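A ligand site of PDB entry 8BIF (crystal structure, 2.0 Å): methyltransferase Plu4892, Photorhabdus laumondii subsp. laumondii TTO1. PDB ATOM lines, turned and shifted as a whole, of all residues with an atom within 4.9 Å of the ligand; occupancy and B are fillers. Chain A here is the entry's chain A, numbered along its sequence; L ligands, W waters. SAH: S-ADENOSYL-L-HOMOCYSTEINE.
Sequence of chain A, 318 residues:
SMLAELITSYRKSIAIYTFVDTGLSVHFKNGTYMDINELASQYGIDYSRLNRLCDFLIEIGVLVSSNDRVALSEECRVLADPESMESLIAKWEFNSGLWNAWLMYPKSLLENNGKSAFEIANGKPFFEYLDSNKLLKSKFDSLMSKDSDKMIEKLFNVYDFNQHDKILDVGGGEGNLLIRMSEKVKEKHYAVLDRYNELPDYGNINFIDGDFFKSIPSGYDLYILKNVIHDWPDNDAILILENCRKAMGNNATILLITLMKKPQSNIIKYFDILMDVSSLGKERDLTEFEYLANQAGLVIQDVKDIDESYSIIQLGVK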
ATOM      1  N   PHE A 127       4.711   3.749  13.100  1.00  0.00           N
ATOM      2  CA  PHE A 127       5.005   5.118  12.601  1.00  0.00           C
ATOM      3  C   PHE A 127       4.685   5.259  11.101  1.00  0.00           C
ATOM      4  O   PHE A 127       4.397   6.397  10.691  1.00  0.00           O
ATOM      5  CB  PHE A 127       6.435   5.534  12.974  1.00  0.00           C
ATOM      6  CG  PHE A 127       6.606   5.760  14.456  1.00  0.00           C
ATOM      7  CD1 PHE A 127       5.883   6.741  15.105  1.00  0.00           C
ATOM      8  CD2 PHE A 127       7.452   4.946  15.204  1.00  0.00           C
ATOM      9  CE1 PHE A 127       6.020   6.928  16.476  1.00  0.00           C
ATOM     10  CE2 PHE A 127       7.593   5.142  16.573  1.00  0.00           C
ATOM     11  CZ  PHE A 127       6.878   6.138  17.207  1.00  0.00           C
ATOM     12  N   PHE A 140      -1.986  11.646  18.424  1.00  0.00           N
ATOM     13  CA  PHE A 140      -0.763  11.067  19.043  1.00  0.00           C
ATOM     14  C   PHE A 140       0.194  12.215  19.404  1.00  0.00           C
ATOM     15  O   PHE A 140       0.650  12.270  20.558  1.00  0.00           O
ATOM     16  CB  PHE A 140      -0.097  10.054  18.115  1.00  0.00           C
ATOM     17  CG  PHE A 140       1.213   9.512  18.629  1.00  0.00           C
ATOM     18  CD1 PHE A 140       1.250   8.434  19.499  1.00  0.00           C
ATOM     19  CD2 PHE A 140       2.420  10.088  18.247  1.00  0.00           C
ATOM     20  CE1 PHE A 140       2.459   7.941  19.966  1.00  0.00           C
ATOM     21  CE2 PHE A 140       3.625   9.587  18.717  1.00  0.00           C
ATOM     22  CZ  PHE A 140       3.646   8.511  19.571  1.00  0.00           C
ATOM     23  N   ASP A 141       0.480  13.080  18.434  1.00  0.00           N
ATOM     24  CA  ASP A 141       1.402  14.233  18.559  1.00  0.00           C
ATOM     25  C   ASP A 141       0.954  15.135  19.730  1.00  0.00           C
ATOM     26  O   ASP A 141       1.821  15.528  20.532  1.00  0.00           O
ATOM     27  CB  ASP A 141       1.505  15.022  17.247  1.00  0.00           C
ATOM     28  CG  ASP A 141       2.368  14.362  16.189  1.00  0.00           C
ATOM     29  OD1 ASP A 141       3.019  13.337  16.490  1.00  0.00           O
ATOM     30  OD2 ASP A 141       2.385  14.879  15.053  1.00  0.00           O
ATOM     31  N   MET A 144       1.756  13.460  23.075  1.00  0.00           N
ATOM     32  CA  MET A 144       3.231  13.556  23.322  1.00  0.00           C
ATOM     33  C   MET A 144       3.565  14.972  23.825  1.00  0.00           C
ATOM     34  O   MET A 144       4.345  15.077  24.787  1.00  0.00           O
ATOM     35  CB  MET A 144       4.051  13.259  22.064  1.00  0.00           C
ATOM     36  CG  MET A 144       3.909  11.836  21.535  1.00  0.00           C
ATOM     37  SD  MET A 144       4.395  10.537  22.707  1.00  0.00           S
ATOM     38  CE  MET A 144       2.784  10.072  23.350  1.00  0.00           C
ATOM     39  N   SER A 145       3.000  16.011  23.214  1.00  0.00           N
ATOM     40  CA  SER A 145       3.218  17.430  23.597  1.00  0.00           C
ATOM     41  C   SER A 145       2.796  17.654  25.053  1.00  0.00           C
ATOM     42  O   SER A 145       3.503  18.389  25.770  1.00  0.00           O
ATOM     43  CB  SER A 145       2.504  18.388  22.673  1.00  0.00           C
ATOM     44  OG  SER A 145       3.127  18.409  21.395  1.00  0.00           O
ATOM     45  N   ASP A 147       2.837  15.483  27.459  1.00  0.00           N
ATOM     46  CA  ASP A 147       3.886  14.830  28.286  1.00  0.00           C
ATOM     47  C   ASP A 147       5.015  15.837  28.545  1.00  0.00           C
ATOM     48  O   ASP A 147       5.488  15.904  29.689  1.00  0.00           O
ATOM     49  CB  ASP A 147       4.391  13.535  27.630  1.00  0.00           C
ATOM     50  CG  ASP A 147       5.454  12.819  28.449  1.00  0.00           C
ATOM     51  OD1 ASP A 147       5.099  11.882  29.174  1.00  0.00           O
ATOM     52  OD2 ASP A 147       6.620  13.222  28.346  1.00  0.00           O
ATOM     53  N   SER A 148       5.416  16.595  27.516  1.00  0.00           N
ATOM     54  CA  SER A 148       6.456  17.649  27.613  1.00  0.00           C
ATOM     55  C   SER A 148       5.984  18.779  28.527  1.00  0.00           C
ATOM     56  O   SER A 148       6.811  19.274  29.318  1.00  0.00           O
ATOM     57  CB  SER A 148       6.851  18.171  26.246  1.00  0.00           C
ATOM     58  OG  SER A 148       7.689  17.229  25.583  1.00  0.00           O
ATOM     59  N   ASP A 169      16.087  18.620  18.940  1.00  0.00           N
ATOM     60  CA  ASP A 169      15.105  17.675  19.526  1.00  0.00           C
ATOM     61  C   ASP A 169      14.906  16.527  18.534  1.00  0.00           C
ATOM     62  O   ASP A 169      14.140  16.705  17.572  1.00  0.00           O
ATOM     63  CB  ASP A 169      13.816  18.412  19.873  1.00  0.00           C
ATOM     64  CG  ASP A 169      12.805  17.645  20.704  1.00  0.00           C
ATOM     65  OD1 ASP A 169      13.133  16.520  21.139  1.00  0.00           O
ATOM     66  OD2 ASP A 169      11.701  18.180  20.909  1.00  0.00           O
ATOM     67  N   GLY A 171      13.470  13.355  17.070  1.00  0.00           N
ATOM     68  CA  GLY A 171      12.114  12.775  17.220  1.00  0.00           C
ATOM     69  C   GLY A 171      11.252  13.622  18.148  1.00  0.00           C
ATOM     70  O   GLY A 171      10.585  13.037  19.012  1.00  0.00           O
ATOM     71  N   GLY A 172      11.251  14.938  17.956  1.00  0.00           N
ATOM     72  CA  GLY A 172      10.554  15.900  18.821  1.00  0.00           C
ATOM     73  C   GLY A 172       9.105  16.153  18.424  1.00  0.00           C
ATOM     74  O   GLY A 172       8.425  16.908  19.161  1.00  0.00           O
ATOM     75  N   GLY A 173       8.631  15.575  17.320  1.00  0.00           N
ATOM     76  CA  GLY A 173       7.243  15.735  16.839  1.00  0.00           C
ATOM     77  C   GLY A 173       6.873  17.201  16.653  1.00  0.00           C
ATOM     78  O   GLY A 173       7.537  17.872  15.854  1.00  0.00           O
ATOM     79  N   LEU A 193      13.982  17.380  14.689  1.00  0.00           N
ATOM     80  CA  LEU A 193      14.014  16.324  13.645  1.00  0.00           C
ATOM     81  C   LEU A 193      12.841  15.370  13.875  1.00  0.00           C
ATOM     82  O   LEU A 193      12.731  14.820  14.995  1.00  0.00           O
ATOM     83  CB  LEU A 193      15.345  15.580  13.696  1.00  0.00           C
ATOM     84  CG  LEU A 193      15.516  14.461  12.667  1.00  0.00           C
ATOM     85  CD1 LEU A 193      15.657  15.043  11.263  1.00  0.00           C
ATOM     86  CD2 LEU A 193      16.708  13.582  12.998  1.00  0.00           C
ATOM     87  N   ASP A 194      12.002  15.176  12.868  1.00  0.00           N
ATOM     88  CA  ASP A 194      10.941  14.128  12.883  1.00  0.00           C
ATOM     89  C   ASP A 194      10.538  13.827  11.438  1.00  0.00           C
ATOM     90  O   ASP A 194      11.158  14.383  10.521  1.00  0.00           O
ATOM     91  CB  ASP A 194       9.750  14.565  13.742  1.00  0.00           C
ATOM     92  CG  ASP A 194       9.085  13.407  14.463  1.00  0.00           C
ATOM     93  OD1 ASP A 194       8.586  12.495  13.773  1.00  0.00           O
ATOM     94  OD2 ASP A 194       9.095  13.422  15.709  1.00  0.00           O
ATOM     95  N   ARG A 195       9.553  12.944  11.269  1.00  0.00           N
ATOM     96  CA  ARG A 195       8.921  12.640   9.964  1.00  0.00           C
ATOM     97  C   ARG A 195       7.661  13.504   9.842  1.00  0.00           C
ATOM     98  O   ARG A 195       6.791  13.380  10.710  1.00  0.00           O
ATOM     99  CB  ARG A 195       8.623  11.144   9.872  1.00  0.00           C
ATOM    100  CG  ARG A 195       9.856  10.270  10.036  1.00  0.00           C
ATOM    101  CD  ARG A 195       9.522   8.795  10.049  1.00  0.00           C
ATOM    102  NE  ARG A 195       8.831   8.397   8.840  1.00  0.00           N
ATOM    103  CZ  ARG A 195       8.251   7.221   8.647  1.00  0.00           C
ATOM    104  NH1 ARG A 195       8.260   6.295   9.587  1.00  0.00           N
ATOM    105  NH2 ARG A 195       7.637   6.972   7.487  1.00  0.00           N
ATOM    106  N   GLY A 210      13.110  14.437   8.311  1.00  0.00           N
ATOM    107  CA  GLY A 210      14.197  13.459   8.128  1.00  0.00           C
ATOM    108  C   GLY A 210      13.837  12.094   8.667  1.00  0.00           C
ATOM    109  O   GLY A 210      12.646  11.750   8.702  1.00  0.00           O
ATOM    110  N   ASP A 211      14.863  11.346   9.071  1.00  0.00           N
ATOM    111  CA  ASP A 211      14.767   9.927   9.475  1.00  0.00           C
ATOM    112  C   ASP A 211      16.026   9.610  10.289  1.00  0.00           C
ATOM    113  O   ASP A 211      17.105   9.577   9.687  1.00  0.00           O
ATOM    114  CB  ASP A 211      14.612   9.029   8.242  1.00  0.00           C
ATOM    115  CG  ASP A 211      14.443   7.556   8.544  1.00  0.00           C
ATOM    116  OD1 ASP A 211      14.074   6.813   7.604  1.00  0.00           O
ATOM    117  OD2 ASP A 211      14.681   7.143   9.703  1.00  0.00           O
ATOM    118  N   PHE A 212      15.902   9.409  11.606  1.00  0.00           N
ATOM    119  CA  PHE A 212      17.081   9.238  12.514  1.00  0.00           C
ATOM    120  C   PHE A 212      17.775   7.888  12.259  1.00  0.00           C
ATOM    121  O   PHE A 212      18.878   7.713  12.798  1.00  0.00           O
ATOM    122  CB  PHE A 212      16.735   9.482  13.989  1.00  0.00           C
ATOM    123  CG  PHE A 212      15.509   8.819  14.559  1.00  0.00           C
ATOM    124  CD1 PHE A 212      15.228   7.476  14.320  1.00  0.00           C
ATOM    125  CD2 PHE A 212      14.678   9.522  15.414  1.00  0.00           C
ATOM    126  CE1 PHE A 212      14.119   6.881  14.899  1.00  0.00           C
ATOM    127  CE2 PHE A 212      13.565   8.918  15.996  1.00  0.00           C
ATOM    128  CZ  PHE A 212      13.289   7.598  15.728  1.00  0.00           C
ATOM    129  N   PHE A 213      17.182   6.997  11.468  1.00  0.00           N
ATOM    130  CA  PHE A 213      17.814   5.720  11.024  1.00  0.00           C
ATOM    131  C   PHE A 213      18.781   5.968   9.861  1.00  0.00           C
ATOM    132  O   PHE A 213      19.692   5.147   9.665  1.00  0.00           O
ATOM    133  CB  PHE A 213      16.763   4.671  10.643  1.00  0.00           C
ATOM    134  CG  PHE A 213      15.908   4.205  11.785  1.00  0.00           C
ATOM    135  CD1 PHE A 213      16.492   3.659  12.927  1.00  0.00           C
ATOM    136  CD2 PHE A 213      14.531   4.289  11.731  1.00  0.00           C
ATOM    137  CE1 PHE A 213      15.698   3.234  13.981  1.00  0.00           C
ATOM    138  CE2 PHE A 213      13.747   3.860  12.787  1.00  0.00           C
ATOM    139  CZ  PHE A 213      14.332   3.329  13.903  1.00  0.00           C
ATOM    140  N   LYS A 226      13.945  12.287  23.693  1.00  0.00           N
ATOM    141  CA  LYS A 226      12.864  12.156  24.707  1.00  0.00           C
ATOM    142  C   LYS A 226      11.817  11.152  24.214  1.00  0.00           C
ATOM    143  O   LYS A 226      11.262  11.388  23.122  1.00  0.00           O
ATOM    144  CB  LYS A 226      12.209  13.505  25.014  1.00  0.00           C
ATOM    145  CG  LYS A 226      11.161  13.463  26.121  1.00  0.00           C
ATOM    146  CD  LYS A 226      10.611  14.820  26.488  1.00  0.00           C
ATOM    147  CE  LYS A 226       9.351  14.744  27.320  1.00  0.00           C
ATOM    148  NZ  LYS A 226       8.174  14.397  26.475  1.00  0.00           N
ATOM    149  N   ASN A 227      11.581  10.092  24.993  1.00  0.00           N
ATOM    150  CA  ASN A 227      10.549   9.046  24.733  1.00  0.00           C
ATOM    151  C   ASN A 227      10.706   8.523  23.299  1.00  0.00           C
ATOM    152  O   ASN A 227       9.679   8.329  22.623  1.00  0.00           O
ATOM    153  CB  ASN A 227       9.143   9.588  25.008  1.00  0.00           C
ATOM    154  CG  ASN A 227       8.928   9.919  26.466  1.00  0.00           C
ATOM    155  OD1 ASN A 227       9.488   9.255  27.344  1.00  0.00           O
ATOM    156  ND2 ASN A 227       8.120  10.932  26.743  1.00  0.00           N
ATOM    157  N   VAL A 228      11.954   8.290  22.865  1.00  0.00           N
ATOM    158  CA  VAL A 228      12.294   7.740  21.518  1.00  0.00           C
ATOM    159  C   VAL A 228      12.838   6.321  21.688  1.00  0.00           C
ATOM    160  O   VAL A 228      12.280   5.400  21.077  1.00  0.00           O
ATOM    161  CB  VAL A 228      13.309   8.642  20.781  1.00  0.00           C
ATOM    162  CG1 VAL A 228      13.883   7.971  19.543  1.00  0.00           C
ATOM    163  CG2 VAL A 228      12.691   9.979  20.410  1.00  0.00           C
ATOM    164  N   ASP A 231      10.895   2.965  22.173  1.00  0.00           N
ATOM    165  CA  ASP A 231      10.054   2.520  21.017  1.00  0.00           C
ATOM    166  C   ASP A 231      10.729   1.382  20.253  1.00  0.00           C
ATOM    167  O   ASP A 231      10.016   0.713  19.480  1.00  0.00           O
ATOM    168  CB  ASP A 231       9.786   3.646  20.023  1.00  0.00           C
ATOM    169  CG  ASP A 231       8.934   4.790  20.547  1.00  0.00           C
ATOM    170  OD1 ASP A 231       8.288   4.614  21.595  1.00  0.00           O
ATOM    171  OD2 ASP A 231       8.922   5.837  19.887  1.00  0.00           O
ATOM    172  N   TRP A 232      12.039   1.169  20.426  1.00  0.00           N
ATOM    173  CA  TRP A 232      12.895   0.453  19.440  1.00  0.00           C
ATOM    174  C   TRP A 232      13.573  -0.773  20.021  1.00  0.00           C
ATOM    175  O   TRP A 232      14.075  -0.734  21.147  1.00  0.00           O
ATOM    176  CB  TRP A 232      13.911   1.429  18.850  1.00  0.00           C
ATOM    177  CG  TRP A 232      13.242   2.577  18.158  1.00  0.00           C
ATOM    178  CD1 TRP A 232      13.232   3.881  18.560  1.00  0.00           C
ATOM    179  CD2 TRP A 232      12.428   2.502  16.975  1.00  0.00           C
ATOM    180  NE1 TRP A 232      12.489   4.632  17.693  1.00  0.00           N
ATOM    181  CE2 TRP A 232      11.977   3.813  16.709  1.00  0.00           C
ATOM    182  CE3 TRP A 232      12.053   1.472  16.113  1.00  0.00           C
ATOM    183  CZ2 TRP A 232      11.171   4.114  15.611  1.00  0.00           C
ATOM    184  CZ3 TRP A 232      11.260   1.762  15.031  1.00  0.00           C
ATOM    185  CH2 TRP A 232      10.824   3.073  14.790  1.00  0.00           C
HETATM  186  N   SAH L   1      10.030  13.379  21.715  1.00  0.00           N
HETATM  187  CA  SAH L   1       8.545  13.603  21.731  1.00  0.00           C
HETATM  188  CB  SAH L   1       7.807  12.508  20.953  1.00  0.00           C
HETATM  189  CG  SAH L   1       8.121  11.097  21.421  1.00  0.00           C
HETATM  190  SD  SAH L   1       7.231   9.817  20.516  1.00  0.00           S
HETATM  191  C   SAH L   1       8.042  13.634  23.175  1.00  0.00           C
HETATM  192  O   SAH L   1       6.972  14.160  23.477  1.00  0.00           O
HETATM  193  OXT SAH L   1       8.696  13.119  24.083  1.00  0.00           O
HETATM  194  C5' SAH L   1       8.461   9.265  19.296  1.00  0.00           C
HETATM  195  C4' SAH L   1       8.718  10.247  18.183  1.00  0.00           C
HETATM  196  O4' SAH L   1       9.686   9.672  17.266  1.00  0.00           O
HETATM  197  C3' SAH L   1       7.500  10.615  17.327  1.00  0.00           C
HETATM  198  O3' SAH L   1       7.358  12.025  17.193  1.00  0.00           O
HETATM  199  C2' SAH L   1       7.803   9.976  15.972  1.00  0.00           C
HETATM  200  O2' SAH L   1       7.249  10.655  14.875  1.00  0.00           O
HETATM  201  C1' SAH L   1       9.326  10.051  15.966  1.00  0.00           C
HETATM  202  N9  SAH L   1       9.959   9.160  14.988  1.00  0.00           N
HETATM  203  C8  SAH L   1       9.627   7.862  14.713  1.00  0.00           C
HETATM  204  N7  SAH L   1      10.364   7.328  13.770  1.00  0.00           N
HETATM  205  C5  SAH L   1      11.235   8.333  13.400  1.00  0.00           C
HETATM  206  C6  SAH L   1      12.272   8.388  12.448  1.00  0.00           C
HETATM  207  N6  SAH L   1      12.606   7.378  11.648  1.00  0.00           N
HETATM  208  N1  SAH L   1      12.953   9.550  12.331  1.00  0.00           N
HETATM  209  C2  SAH L   1      12.608  10.584  13.119  1.00  0.00           C
HETATM  210  N3  SAH L   1      11.658  10.643  14.048  1.00  0.00           N
HETATM  211  C4  SAH L   1      10.996   9.477  14.138  1.00  0.00           C
HETATM  212  O   HOH W   1       7.329   6.984  22.541  1.00  0.00           O
HETATM  213  O   HOH W   2      10.656   6.993  18.088  1.00  0.00           O
HETATM  214  O   HOH W   3       5.054  13.240  18.439  1.00  0.00           O
HETATM  215  O   HOH W   4       6.104  11.948  25.089  1.00  0.00           O
HETATM  216  O   HOH W   5       4.841  12.381  14.910  1.00  0.00           O
HETATM  217  O   HOH W   6      10.089   5.532  11.764  1.00  0.00           O
HETATM  218  O   HOH W   7       6.910  16.766  23.154  1.00  0.00           O
HETATM  219  O   HOH W   8      13.181  13.852  21.298  1.00  0.00           O
HETATM  220  O   HOH W   9      10.661  15.931  22.620  1.00  0.00           O
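N of Phe 212 lies within hydrogen-bond range of N1 of the ligand (3.0 Å).
The backbone carbonyl oxygen (O) of Gly 171 is in hydrogen-bond range of a nitrogen (N) of the ligand, 2.8 Å away.
The side-chain amino group (NZ) of Lys 226 is in salt-bridge range of an oxygen (OXT) of the ligand, 2.8 Å away.
N of the ligand sits at hydrogen-bond distance from O of Lys 226, 2.7 Å away.
An oxygen (O2') of the ligand is in hydrogen-bond range of the side-chain carboxylate (OD1) of Asp 194 (2.5 Å).
An oxygen (OXT) of the ligand lies within hydrogen-bond range of the side-chain amide nitrogen (ND2) of Asn 227 (3.5 Å).
The backbone carbonyl oxygen of Met 144 lies close to an oxygen (O) of the ligand (3.1 Å).
OD2 of Asp 211 lies within hydrogen-bond range of N6 of the ligand, 2.9 Å away.
The backbone NH (N) of Gly 171 lies within hydrogen-bond range of the backbone carbonyl oxygen (O) of Leu 193 (2.6 Å).
OG of Ser 148 is in hydrogen-bond range of NZ of Lys 226, 3.0 Å away.
The side-chain carboxylate of Asp 147 is in salt-bridge range of the side-chain amino group of Lys 226.
The backbone carbonyl oxygen of Asp 194 sits at hydrogen-bond distance from the backbone NH of Gly 210.
The backbone NH of Gly 173 is in hydrogen-bond range of the side-chain carboxylate of Asp 194 (2.7 Å).
The side-chain carboxylate of Asp 211 sits at hydrogen-bond distance from the backbone NH of Phe 213, at 3.1 Å.
The indole nitrogen of Trp 232 sits close to the backbone carbonyl oxygen of Val 228, at 3.5 Å.
ND2 of Asn 227 sits close to NZ of Lys 226 (3.5 Å).
CE1 of Phe 127 touches C2' of the ligand, at 3.6 Å.
CZ of Phe 140 touches SD of the ligand, 3.9 Å away.
Ser 148 touches the ligand.
Gly 172 touches the ligand (CA to N, 3.9 Å).
CA of Gly 173 touches O3' of the ligand, 3.7 Å away.
CD of Arg 195 touches C6 of the ligand (3.7 Å).
Phe 213 touches the ligand.
OD2 of Asp 231 touches C5' of the ligand (3.5 Å).
Trp 232 touches the ligand.
Hydrophobic or aromatic side chains within 4 Å of the ligand: Phe 127, Phe 140, Met 144, Phe 212, Phe 213 and Trp 232.
16 residues have an atom within 4 Å of the ligand: Phe 127, Phe 140, Met 144, Ser 148, Gly 171, Gly 172, Gly 173, Asp 194, Arg 195, Asp 211, Phe 212, Phe 213, Lys 226, Asn 227, Asp 231 and Trp 232.
Water W7 lies within hydrogen-bond range of OG of Ser 148 (2.6 Å), O of the ligand (2.6 Å) and O of Met 144 (3.5 Å).
Water W6 bridges a nitrogen (N7) of the ligand (2.7 Å) and the guanidinium group (NH1) of Arg 195 (2.9 Å).
Water W9 bridges N of the ligand (2.8 Å) and OD1 of Asp 169 (2.9 Å).
Water W4 lies within hydrogen-bond range of ND2 of Asn 227, O of the ligand, SD of Met 144 and NZ of Lys 226.
Water W3 bridges OD1 of Asp 141 and O3' of the ligand.
Water W2 lies within hydrogen-bond range of OD2 of Asp 231 (2.8 Å), O4' of the ligand (3.0 Å) and NE1 of Trp 232 (3.0 Å).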
